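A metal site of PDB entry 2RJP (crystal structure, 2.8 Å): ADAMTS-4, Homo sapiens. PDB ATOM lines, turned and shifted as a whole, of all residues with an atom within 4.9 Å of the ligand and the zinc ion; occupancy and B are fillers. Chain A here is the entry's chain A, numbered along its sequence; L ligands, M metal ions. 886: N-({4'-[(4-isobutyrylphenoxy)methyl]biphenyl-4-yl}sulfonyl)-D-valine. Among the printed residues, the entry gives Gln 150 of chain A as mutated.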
ATOM      1  N   ALA A  36     -13.241  34.674 -27.556  1.00  0.00           N
ATOM      2  CA  ALA A  36     -13.643  33.325 -27.175  1.00  0.00           C
ATOM      3  C   ALA A  36     -15.026  33.332 -26.526  1.00  0.00           C
ATOM      4  O   ALA A  36     -15.881  32.536 -26.895  1.00  0.00           O
ATOM      5  CB  ALA A  36     -12.617  32.704 -26.252  1.00  0.00           C
ATOM      6  N   ALA A  40     -18.673  31.423 -27.954  1.00  0.00           N
ATOM      7  CA  ALA A  40     -19.595  30.549 -27.237  1.00  0.00           C
ATOM      8  C   ALA A  40     -21.045  30.989 -27.466  1.00  0.00           C
ATOM      9  O   ALA A  40     -21.923  30.146 -27.650  1.00  0.00           O
ATOM     10  CB  ALA A  40     -19.260  30.493 -25.743  1.00  0.00           C
ATOM     11  N   ASP A 116     -12.464  28.849  -4.294  1.00  0.00           N
ATOM     12  CA  ASP A 116     -12.625  28.233  -5.628  1.00  0.00           C
ATOM     13  C   ASP A 116     -13.543  29.055  -6.542  1.00  0.00           C
ATOM     14  O   ASP A 116     -13.548  28.849  -7.758  1.00  0.00           O
ATOM     15  CB  ASP A 116     -13.148  26.798  -5.495  1.00  0.00           C
ATOM     16  CG  ASP A 116     -12.204  25.885  -4.699  1.00  0.00           C
ATOM     17  OD1 ASP A 116     -10.969  26.058  -4.801  1.00  0.00           O
ATOM     18  OD2 ASP A 116     -12.697  24.997  -3.977  1.00  0.00           O
ATOM     19  N   THR A 117     -14.310  29.964  -5.956  1.00  0.00           N
ATOM     20  CA  THR A 117     -15.101  30.931  -6.724  1.00  0.00           C
ATOM     21  C   THR A 117     -14.256  31.588  -7.817  1.00  0.00           C
ATOM     22  O   THR A 117     -13.143  32.051  -7.545  1.00  0.00           O
ATOM     23  CB  THR A 117     -15.679  32.012  -5.788  1.00  0.00           C
ATOM     24  OG1 THR A 117     -16.508  31.396  -4.808  1.00  0.00           O
ATOM     25  CG2 THR A 117     -16.485  33.052  -6.553  1.00  0.00           C
ATOM     26  N   LEU A 118     -14.773  31.605  -9.040  1.00  0.00           N
ATOM     27  CA  LEU A 118     -14.048  32.195 -10.171  1.00  0.00           C
ATOM     28  C   LEU A 118     -14.709  33.456 -10.748  1.00  0.00           C
ATOM     29  O   LEU A 118     -14.111  34.142 -11.572  1.00  0.00           O
ATOM     30  CB  LEU A 118     -13.785  31.154 -11.259  1.00  0.00           C
ATOM     31  CG  LEU A 118     -12.656  30.152 -10.952  1.00  0.00           C
ATOM     32  CD1 LEU A 118     -12.584  29.054 -11.979  1.00  0.00           C
ATOM     33  CD2 LEU A 118     -11.304  30.850 -10.844  1.00  0.00           C
ATOM     34  N   GLY A 119     -15.929  33.752 -10.317  1.00  0.00           N
ATOM     35  CA  GLY A 119     -16.619  34.951 -10.783  1.00  0.00           C
ATOM     36  C   GLY A 119     -18.014  35.092 -10.211  1.00  0.00           C
ATOM     37  O   GLY A 119     -18.498  34.203  -9.533  1.00  0.00           O
ATOM     38  N   MET A 120     -18.655  36.215 -10.499  1.00  0.00           N
ATOM     39  CA  MET A 120     -19.969  36.497  -9.912  1.00  0.00           C
ATOM     40  C   MET A 120     -20.782  37.450 -10.780  1.00  0.00           C
ATOM     41  O   MET A 120     -20.249  38.368 -11.385  1.00  0.00           O
ATOM     42  CB  MET A 120     -19.811  37.058  -8.490  1.00  0.00           C
ATOM     43  CG  MET A 120     -21.058  36.945  -7.649  1.00  0.00           C
ATOM     44  SD  MET A 120     -20.800  37.303  -5.901  1.00  0.00           S
ATOM     45  CE  MET A 120     -20.912  35.688  -5.153  1.00  0.00           C
ATOM     46  N   PHE A 145     -14.168  31.275 -20.546  1.00  0.00           N
ATOM     47  CA  PHE A 145     -15.241  30.375 -20.151  1.00  0.00           C
ATOM     48  C   PHE A 145     -15.980  30.885 -18.920  1.00  0.00           C
ATOM     49  O   PHE A 145     -17.205  30.778 -18.841  1.00  0.00           O
ATOM     50  CB  PHE A 145     -14.684  28.971 -19.926  1.00  0.00           C
ATOM     51  CG  PHE A 145     -13.913  28.441 -21.117  1.00  0.00           C
ATOM     52  CD1 PHE A 145     -14.075  28.995 -22.389  1.00  0.00           C
ATOM     53  CD2 PHE A 145     -13.046  27.362 -20.968  1.00  0.00           C
ATOM     54  CE1 PHE A 145     -13.370  28.500 -23.495  1.00  0.00           C
ATOM     55  CE2 PHE A 145     -12.333  26.858 -22.067  1.00  0.00           C
ATOM     56  CZ  PHE A 145     -12.496  27.416 -23.330  1.00  0.00           C
ATOM     57  N   THR A 146     -15.257  31.448 -17.955  1.00  0.00           N
ATOM     58  CA  THR A 146     -15.882  32.010 -16.759  1.00  0.00           C
ATOM     59  C   THR A 146     -16.779  33.171 -17.178  1.00  0.00           C
ATOM     60  O   THR A 146     -17.895  33.329 -16.665  1.00  0.00           O
ATOM     61  CB  THR A 146     -14.830  32.481 -15.738  1.00  0.00           C
ATOM     62  OG1 THR A 146     -13.805  31.493 -15.616  1.00  0.00           O
ATOM     63  CG2 THR A 146     -15.455  32.727 -14.377  1.00  0.00           C
ATOM     64  N   ALA A 148     -18.220  33.717 -20.263  1.00  0.00           N
ATOM     65  CA  ALA A 148     -19.414  33.205 -20.959  1.00  0.00           C
ATOM     66  C   ALA A 148     -20.459  32.731 -19.965  1.00  0.00           C
ATOM     67  O   ALA A 148     -21.662  32.938 -20.152  1.00  0.00           O
ATOM     68  CB  ALA A 148     -19.035  32.066 -21.905  1.00  0.00           C
ATOM     69  N   HIS A 149     -19.998  32.081 -18.894  1.00  0.00           N
ATOM     70  CA  HIS A 149     -20.872  31.611 -17.830  1.00  0.00           C
ATOM     71  C   HIS A 149     -21.528  32.797 -17.115  1.00  0.00           C
ATOM     72  O   HIS A 149     -22.738  32.813 -16.906  1.00  0.00           O
ATOM     73  CB  HIS A 149     -20.064  30.743 -16.848  1.00  0.00           C
ATOM     74  CG  HIS A 149     -20.833  30.262 -15.657  1.00  0.00           C
ATOM     75  ND1 HIS A 149     -21.324  28.985 -15.561  1.00  0.00           N
ATOM     76  CD2 HIS A 149     -21.177  30.881 -14.507  1.00  0.00           C
ATOM     77  CE1 HIS A 149     -21.943  28.834 -14.405  1.00  0.00           C
ATOM     78  NE2 HIS A 149     -21.864  29.972 -13.746  1.00  0.00           N
ATOM     79  N   GLN A 150     -20.709  33.802 -16.776  1.00  0.00           N
ATOM     80  CA  GLN A 150     -21.164  34.978 -16.047  1.00  0.00           C
ATOM     81  C   GLN A 150     -22.181  35.786 -16.831  1.00  0.00           C
ATOM     82  O   GLN A 150     -23.167  36.271 -16.261  1.00  0.00           O
ATOM     83  CB  GLN A 150     -19.995  35.859 -15.619  1.00  0.00           C
ATOM     84  CG  GLN A 150     -19.062  35.245 -14.587  1.00  0.00           C
ATOM     85  CD  GLN A 150     -19.783  34.711 -13.348  1.00  0.00           C
ATOM     86  OE1 GLN A 150     -20.832  35.215 -12.960  1.00  0.00           O
ATOM     87  NE2 GLN A 150     -19.203  33.688 -12.720  1.00  0.00           N
ATOM     88  N   HIS A 153     -25.520  34.050 -16.689  1.00  0.00           N
ATOM     89  CA  HIS A 153     -26.283  34.538 -15.553  1.00  0.00           C
ATOM     90  C   HIS A 153     -26.937  35.899 -15.873  1.00  0.00           C
ATOM     91  O   HIS A 153     -28.143  36.076 -15.662  1.00  0.00           O
ATOM     92  CB  HIS A 153     -25.403  34.663 -14.295  1.00  0.00           C
ATOM     93  CG  HIS A 153     -25.139  33.362 -13.596  1.00  0.00           C
ATOM     94  ND1 HIS A 153     -26.144  32.533 -13.149  1.00  0.00           N
ATOM     95  CD2 HIS A 153     -23.979  32.772 -13.213  1.00  0.00           C
ATOM     96  CE1 HIS A 153     -25.612  31.483 -12.548  1.00  0.00           C
ATOM     97  NE2 HIS A 153     -24.306  31.602 -12.574  1.00  0.00           N
ATOM     98  N   HIS A 159     -28.116  27.648 -13.044  1.00  0.00           N
ATOM     99  CA  HIS A 159     -27.228  26.496 -13.175  1.00  0.00           C
ATOM    100  C   HIS A 159     -27.970  25.242 -13.651  1.00  0.00           C
ATOM    101  O   HIS A 159     -29.181  25.144 -13.484  1.00  0.00           O
ATOM    102  CB  HIS A 159     -26.522  26.213 -11.843  1.00  0.00           C
ATOM    103  CG  HIS A 159     -25.438  27.184 -11.513  1.00  0.00           C
ATOM    104  ND1 HIS A 159     -25.053  27.446 -10.224  1.00  0.00           N
ATOM    105  CD2 HIS A 159     -24.674  27.973 -12.299  1.00  0.00           C
ATOM    106  CE1 HIS A 159     -24.083  28.334 -10.224  1.00  0.00           C
ATOM    107  NE2 HIS A 159     -23.827  28.678 -11.475  1.00  0.00           N
ATOM    108  N   HIS A 177     -21.857  21.412 -19.847  1.00  0.00           N
ATOM    109  CA  HIS A 177     -22.413  22.641 -20.401  1.00  0.00           C
ATOM    110  C   HIS A 177     -21.889  23.877 -19.671  1.00  0.00           C
ATOM    111  O   HIS A 177     -21.422  23.772 -18.545  1.00  0.00           O
ATOM    112  CB  HIS A 177     -23.939  22.601 -20.372  1.00  0.00           C
ATOM    113  CG  HIS A 177     -24.513  21.347 -20.916  1.00  0.00           C
ATOM    114  ND1 HIS A 177     -24.501  21.032 -22.264  1.00  0.00           N
ATOM    115  CD2 HIS A 177     -25.111  20.295 -20.304  1.00  0.00           C
ATOM    116  CE1 HIS A 177     -25.059  19.862 -22.447  1.00  0.00           C
ATOM    117  NE2 HIS A 177     -25.443  19.385 -21.280  1.00  0.00           N
ATOM    118  N   VAL A 178     -21.991  25.034 -20.323  1.00  0.00           N
ATOM    119  CA  VAL A 178     -21.518  26.306 -19.782  1.00  0.00           C
ATOM    120  C   VAL A 178     -22.083  26.615 -18.389  1.00  0.00           C
ATOM    121  O   VAL A 178     -21.350  27.086 -17.509  1.00  0.00           O
ATOM    122  CB  VAL A 178     -21.818  27.478 -20.762  1.00  0.00           C
ATOM    123  CG1 VAL A 178     -21.357  28.806 -20.185  1.00  0.00           C
ATOM    124  CG2 VAL A 178     -21.153  27.241 -22.111  1.00  0.00           C
ATOM    125  N   MET A 179     -23.367  26.328 -18.195  1.00  0.00           N
ATOM    126  CA  MET A 179     -24.039  26.706 -16.950  1.00  0.00           C
ATOM    127  C   MET A 179     -24.012  25.631 -15.847  1.00  0.00           C
ATOM    128  O   MET A 179     -24.871  25.600 -14.968  1.00  0.00           O
ATOM    129  CB  MET A 179     -25.450  27.250 -17.230  1.00  0.00           C
ATOM    130  CG  MET A 179     -25.467  28.514 -18.102  1.00  0.00           C
ATOM    131  SD  MET A 179     -24.324  29.839 -17.603  1.00  0.00           S
ATOM    132  CE  MET A 179     -25.106  30.472 -16.113  1.00  0.00           C
ATOM    133  N   ALA A 180     -22.998  24.775 -15.915  1.00  0.00           N
ATOM    134  CA  ALA A 180     -22.686  23.815 -14.856  1.00  0.00           C
ATOM    135  C   ALA A 180     -22.326  24.583 -13.576  1.00  0.00           C
ATOM    136  O   ALA A 180     -21.781  25.666 -13.670  1.00  0.00           O
ATOM    137  CB  ALA A 180     -21.539  22.937 -15.285  1.00  0.00           C
ATOM    138  N   PRO A 181     -22.648  24.032 -12.392  1.00  0.00           N
ATOM    139  CA  PRO A 181     -22.336  24.767 -11.148  1.00  0.00           C
ATOM    140  C   PRO A 181     -20.841  24.859 -10.852  1.00  0.00           C
ATOM    141  O   PRO A 181     -20.406  25.762 -10.134  1.00  0.00           O
ATOM    142  CB  PRO A 181     -23.048  23.950 -10.072  1.00  0.00           C
ATOM    143  CG  PRO A 181     -23.148  22.583 -10.629  1.00  0.00           C
ATOM    144  CD  PRO A 181     -23.312  22.736 -12.116  1.00  0.00           C
ATOM    145  N   VAL A 182     -20.064  23.922 -11.399  1.00  0.00           N
ATOM    146  CA  VAL A 182     -18.607  23.954 -11.295  1.00  0.00           C
ATOM    147  C   VAL A 182     -17.973  23.980 -12.680  1.00  0.00           C
ATOM    148  O   VAL A 182     -18.634  23.627 -13.660  1.00  0.00           O
ATOM    149  CB  VAL A 182     -18.035  22.739 -10.514  1.00  0.00           C
ATOM    150  CG1 VAL A 182     -18.473  22.781  -9.056  1.00  0.00           C
ATOM    151  CG2 VAL A 182     -18.430  21.415 -11.210  1.00  0.00           C
ATOM    152  N   MET A 183     -16.712  24.376 -12.764  1.00  0.00           N
ATOM    153  CA  MET A 183     -15.975  24.347 -14.021  1.00  0.00           C
ATOM    154  C   MET A 183     -16.111  22.968 -14.658  1.00  0.00           C
ATOM    155  O   MET A 183     -15.907  21.946 -13.996  1.00  0.00           O
ATOM    156  CB  MET A 183     -14.506  24.695 -13.792  1.00  0.00           C
ATOM    157  CG  MET A 183     -13.659  24.830 -15.066  1.00  0.00           C
ATOM    158  SD  MET A 183     -13.971  26.373 -15.978  1.00  0.00           S
ATOM    159  CE  MET A 183     -12.507  26.468 -17.031  1.00  0.00           C
ATOM    160  N   ALA A 184     -16.478  22.943 -15.927  1.00  0.00           N
ATOM    161  CA  ALA A 184     -16.724  21.695 -16.619  1.00  0.00           C
ATOM    162  C   ALA A 184     -16.092  21.712 -18.000  1.00  0.00           C
ATOM    163  O   ALA A 184     -15.955  22.776 -18.608  1.00  0.00           O
ATOM    164  CB  ALA A 184     -18.205  21.463 -16.742  1.00  0.00           C
ATOM    165  N   VAL A 186     -16.681  21.501 -21.569  1.00  0.00           N
ATOM    166  CA  VAL A 186     -17.927  21.748 -22.282  1.00  0.00           C
ATOM    167  C   VAL A 186     -17.971  21.088 -23.654  1.00  0.00           C
ATOM    168  O   VAL A 186     -16.982  21.093 -24.383  1.00  0.00           O
ATOM    169  CB  VAL A 186     -18.202  23.249 -22.391  1.00  0.00           C
ATOM    170  CG1 VAL A 186     -19.553  23.496 -22.992  1.00  0.00           C
ATOM    171  CG2 VAL A 186     -18.140  23.854 -21.031  1.00  0.00           C
ATOM    172  N   ASP A 187     -19.133  20.524 -23.981  1.00  0.00           N
ATOM    173  CA  ASP A 187     -19.370  19.871 -25.260  1.00  0.00           C
ATOM    174  C   ASP A 187     -19.225  20.880 -26.380  1.00  0.00           C
ATOM    175  O   ASP A 187     -20.016  21.819 -26.462  1.00  0.00           O
ATOM    176  CB  ASP A 187     -20.782  19.266 -25.279  1.00  0.00           C
ATOM    177  CG  ASP A 187     -20.933  18.157 -26.324  1.00  0.00           C
ATOM    178  OD1 ASP A 187     -20.110  18.091 -27.269  1.00  0.00           O
ATOM    179  OD2 ASP A 187     -21.884  17.365 -26.178  1.00  0.00           O
ATOM    180  N   PRO A 188     -18.194  20.721 -27.230  1.00  0.00           N
ATOM    181  CA  PRO A 188     -18.074  21.646 -28.366  1.00  0.00           C
ATOM    182  C   PRO A 188     -19.269  21.559 -29.323  1.00  0.00           C
ATOM    183  O   PRO A 188     -19.625  22.574 -29.947  1.00  0.00           O
ATOM    184  CB  PRO A 188     -16.773  21.210 -29.053  1.00  0.00           C
ATOM    185  CG  PRO A 188     -16.495  19.830 -28.562  1.00  0.00           C
ATOM    186  CD  PRO A 188     -17.112  19.721 -27.197  1.00  0.00           C
ATOM    187  N   PRO A 191     -22.553  23.464 -26.319  1.00  0.00           N
ATOM    188  CA  PRO A 191     -22.100  24.126 -25.093  1.00  0.00           C
ATOM    189  C   PRO A 191     -23.237  24.518 -24.170  1.00  0.00           C
ATOM    190  O   PRO A 191     -23.052  24.563 -22.953  1.00  0.00           O
ATOM    191  CB  PRO A 191     -21.408  25.400 -25.618  1.00  0.00           C
ATOM    192  CG  PRO A 191     -21.268  25.219 -27.080  1.00  0.00           C
ATOM    193  CD  PRO A 191     -22.348  24.299 -27.507  1.00  0.00           C
ATOM    194  N   ASP A 279      -8.166  26.001 -27.731  1.00  0.00           N
ATOM    195  CA  ASP A 279      -8.495  25.678 -29.116  1.00  0.00           C
ATOM    196  C   ASP A 279      -7.435  26.196 -30.063  1.00  0.00           C
ATOM    197  O   ASP A 279      -7.150  27.391 -30.086  1.00  0.00           O
ATOM    198  CB  ASP A 279      -9.838  26.306 -29.491  1.00  0.00           C
ATOM    199  CG  ASP A 279     -11.022  25.594 -28.870  1.00  0.00           C
ATOM    200  OD1 ASP A 279     -10.824  24.597 -28.120  1.00  0.00           O
ATOM    201  OD2 ASP A 279     -12.167  26.045 -29.139  1.00  0.00           O
HETATM  202  C1  886 L   1     -20.173  32.102  -6.466  1.00  0.00           C
HETATM  203  C2  886 L   1     -21.199  31.985  -7.612  1.00  0.00           C
HETATM  204  C3  886 L   1     -21.979  33.306  -7.685  1.00  0.00           C
HETATM  205  C4  886 L   1     -20.481  31.619  -8.926  1.00  0.00           C
HETATM  206  C5  886 L   1     -21.443  31.444 -10.157  1.00  0.00           C
HETATM  207  O1  886 L   1     -22.261  30.491 -10.027  1.00  0.00           O
HETATM  208  O2  886 L   1     -21.310  32.229 -11.119  1.00  0.00           O
HETATM  209  N1  886 L   1     -19.887  30.243  -8.722  1.00  0.00           N
HETATM  210  S1  886 L   1     -18.256  30.022  -9.075  1.00  0.00           S
HETATM  211  O3  886 L   1     -17.785  28.967  -8.180  1.00  0.00           O
HETATM  212  O4  886 L   1     -17.586  31.306  -9.089  1.00  0.00           O
HETATM  213  C6  886 L   1     -18.236  29.411 -10.742  1.00  0.00           C
HETATM  214  C7  886 L   1     -18.552  28.073 -10.979  1.00  0.00           C
HETATM  215  C8  886 L   1     -18.531  27.593 -12.291  1.00  0.00           C
HETATM  216  C9  886 L   1     -18.192  28.427 -13.387  1.00  0.00           C
HETATM  217  C10 886 L   1     -17.882  29.775 -13.112  1.00  0.00           C
HETATM  218  C11 886 L   1     -17.892  30.264 -11.802  1.00  0.00           C
HETATM  219  C12 886 L   1     -18.162  27.885 -14.768  1.00  0.00           C
HETATM  220  C13 886 L   1     -17.343  28.475 -15.758  1.00  0.00           C
HETATM  221  C14 886 L   1     -17.294  27.965 -17.072  1.00  0.00           C
HETATM  222  C15 886 L   1     -18.049  26.836 -17.425  1.00  0.00           C
HETATM  223  C16 886 L   1     -18.859  26.232 -16.437  1.00  0.00           C
HETATM  224  C17 886 L   1     -18.905  26.746 -15.136  1.00  0.00           C
HETATM  225  C18 886 L   1     -18.039  26.264 -18.826  1.00  0.00           C
HETATM  226  O5  886 L   1     -16.912  26.723 -19.579  1.00  0.00           O
HETATM  227  C19 886 L   1     -16.958  27.062 -20.909  1.00  0.00           C
HETATM  228  C20 886 L   1     -17.670  28.101 -21.532  1.00  0.00           C
HETATM  229  C21 886 L   1     -17.561  28.307 -22.926  1.00  0.00           C
HETATM  230  C22 886 L   1     -16.740  27.499 -23.734  1.00  0.00           C
HETATM  231  C23 886 L   1     -16.019  26.477 -23.096  1.00  0.00           C
HETATM  232  C24 886 L   1     -16.126  26.266 -21.711  1.00  0.00           C
HETATM  233  C25 886 L   1     -16.580  27.711 -25.227  1.00  0.00           C
HETATM  234  O6  886 L   1     -16.168  28.823 -25.555  1.00  0.00           O
HETATM  235  C26 886 L   1     -16.515  26.590 -26.278  1.00  0.00           C
HETATM  236  C27 886 L   1     -17.614  25.547 -26.119  1.00  0.00           C
HETATM  237  C28 886 L   1     -15.123  25.966 -26.395  1.00  0.00           C
HETATM  238 ZN    ZN M   1     -22.781  30.316 -11.918  1.00  0.00          ZN
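An oxygen (O2) of the ligand sits close to the side-chain amide nitrogen (NE2) of Gln 150 (3.0 Å). N of Gly 119 lies within hydrogen-bond range of O4 of the ligand, at 3.2 Å. The backbone NH of Leu 118 lies within hydrogen-bond range of an oxygen (O4) of the ligand (2.8 Å).
The backbone carbonyl oxygen (O) of Gly 119 sits close to the side-chain amide nitrogen (NE2) of Gln 150 (3.3 Å). O of Pro 191 sits at hydrogen-bond distance from N of Val 178. The side-chain amide nitrogen (NE2) of Gln 150 sits close to the backbone NH (N) of Met 120, 3.4 Å away. ND1 of His 149 sits at hydrogen-bond distance from O of Val 178. The side-chain sulfur of Met 179 lies within hydrogen-bond range of a ring nitrogen (ND1) of His 149.
Merely in contact with the ligand: Ala 36, Ala 40, Thr 117, Met 120, Phe 145, Thr 146, Val 178, Ala 180, Pro 181, Val 182, Met 183, Val 186 and Pro 191. Hydrophobic or aromatic side chains that line the ligand: Ala 40, Met 120, Phe 145, His 149, His 153, His 159, Val 178, Met 183, Val 186 and Pro 191. 19 residues have an atom within 4 Å of the ligand: Ala 36, Ala 40, Thr 117, Leu 118, Gly 119, Met 120, Phe 145, Thr 146, His 149, Gln 150, His 153, His 159, Val 178, Ala 180, Pro 181, Val 182, Met 183, Val 186 and Pro 191. Along chain A the residues within 4 Å of the ligand span positions 36 to 191. The nearest printed residue that does not touch the ligand is Asp 279 (4.03 Å).
Of the 27 residues printed, 3 come within 4 Å of the zinc ion.
The zinc ion is bound by an oxygen (O1) of the ligand (2.0 Å). NE2 of His 159 binds the zinc ion. The zinc ion is bound by NE2 of His 149, 2.1 Å away. A ring nitrogen (NE2) of His 153 is bound to the zinc ion (2.1 Å). The zinc ion is bound by an oxygen (O2) of the ligand. The zinc ion has five donor atoms within binding distance.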
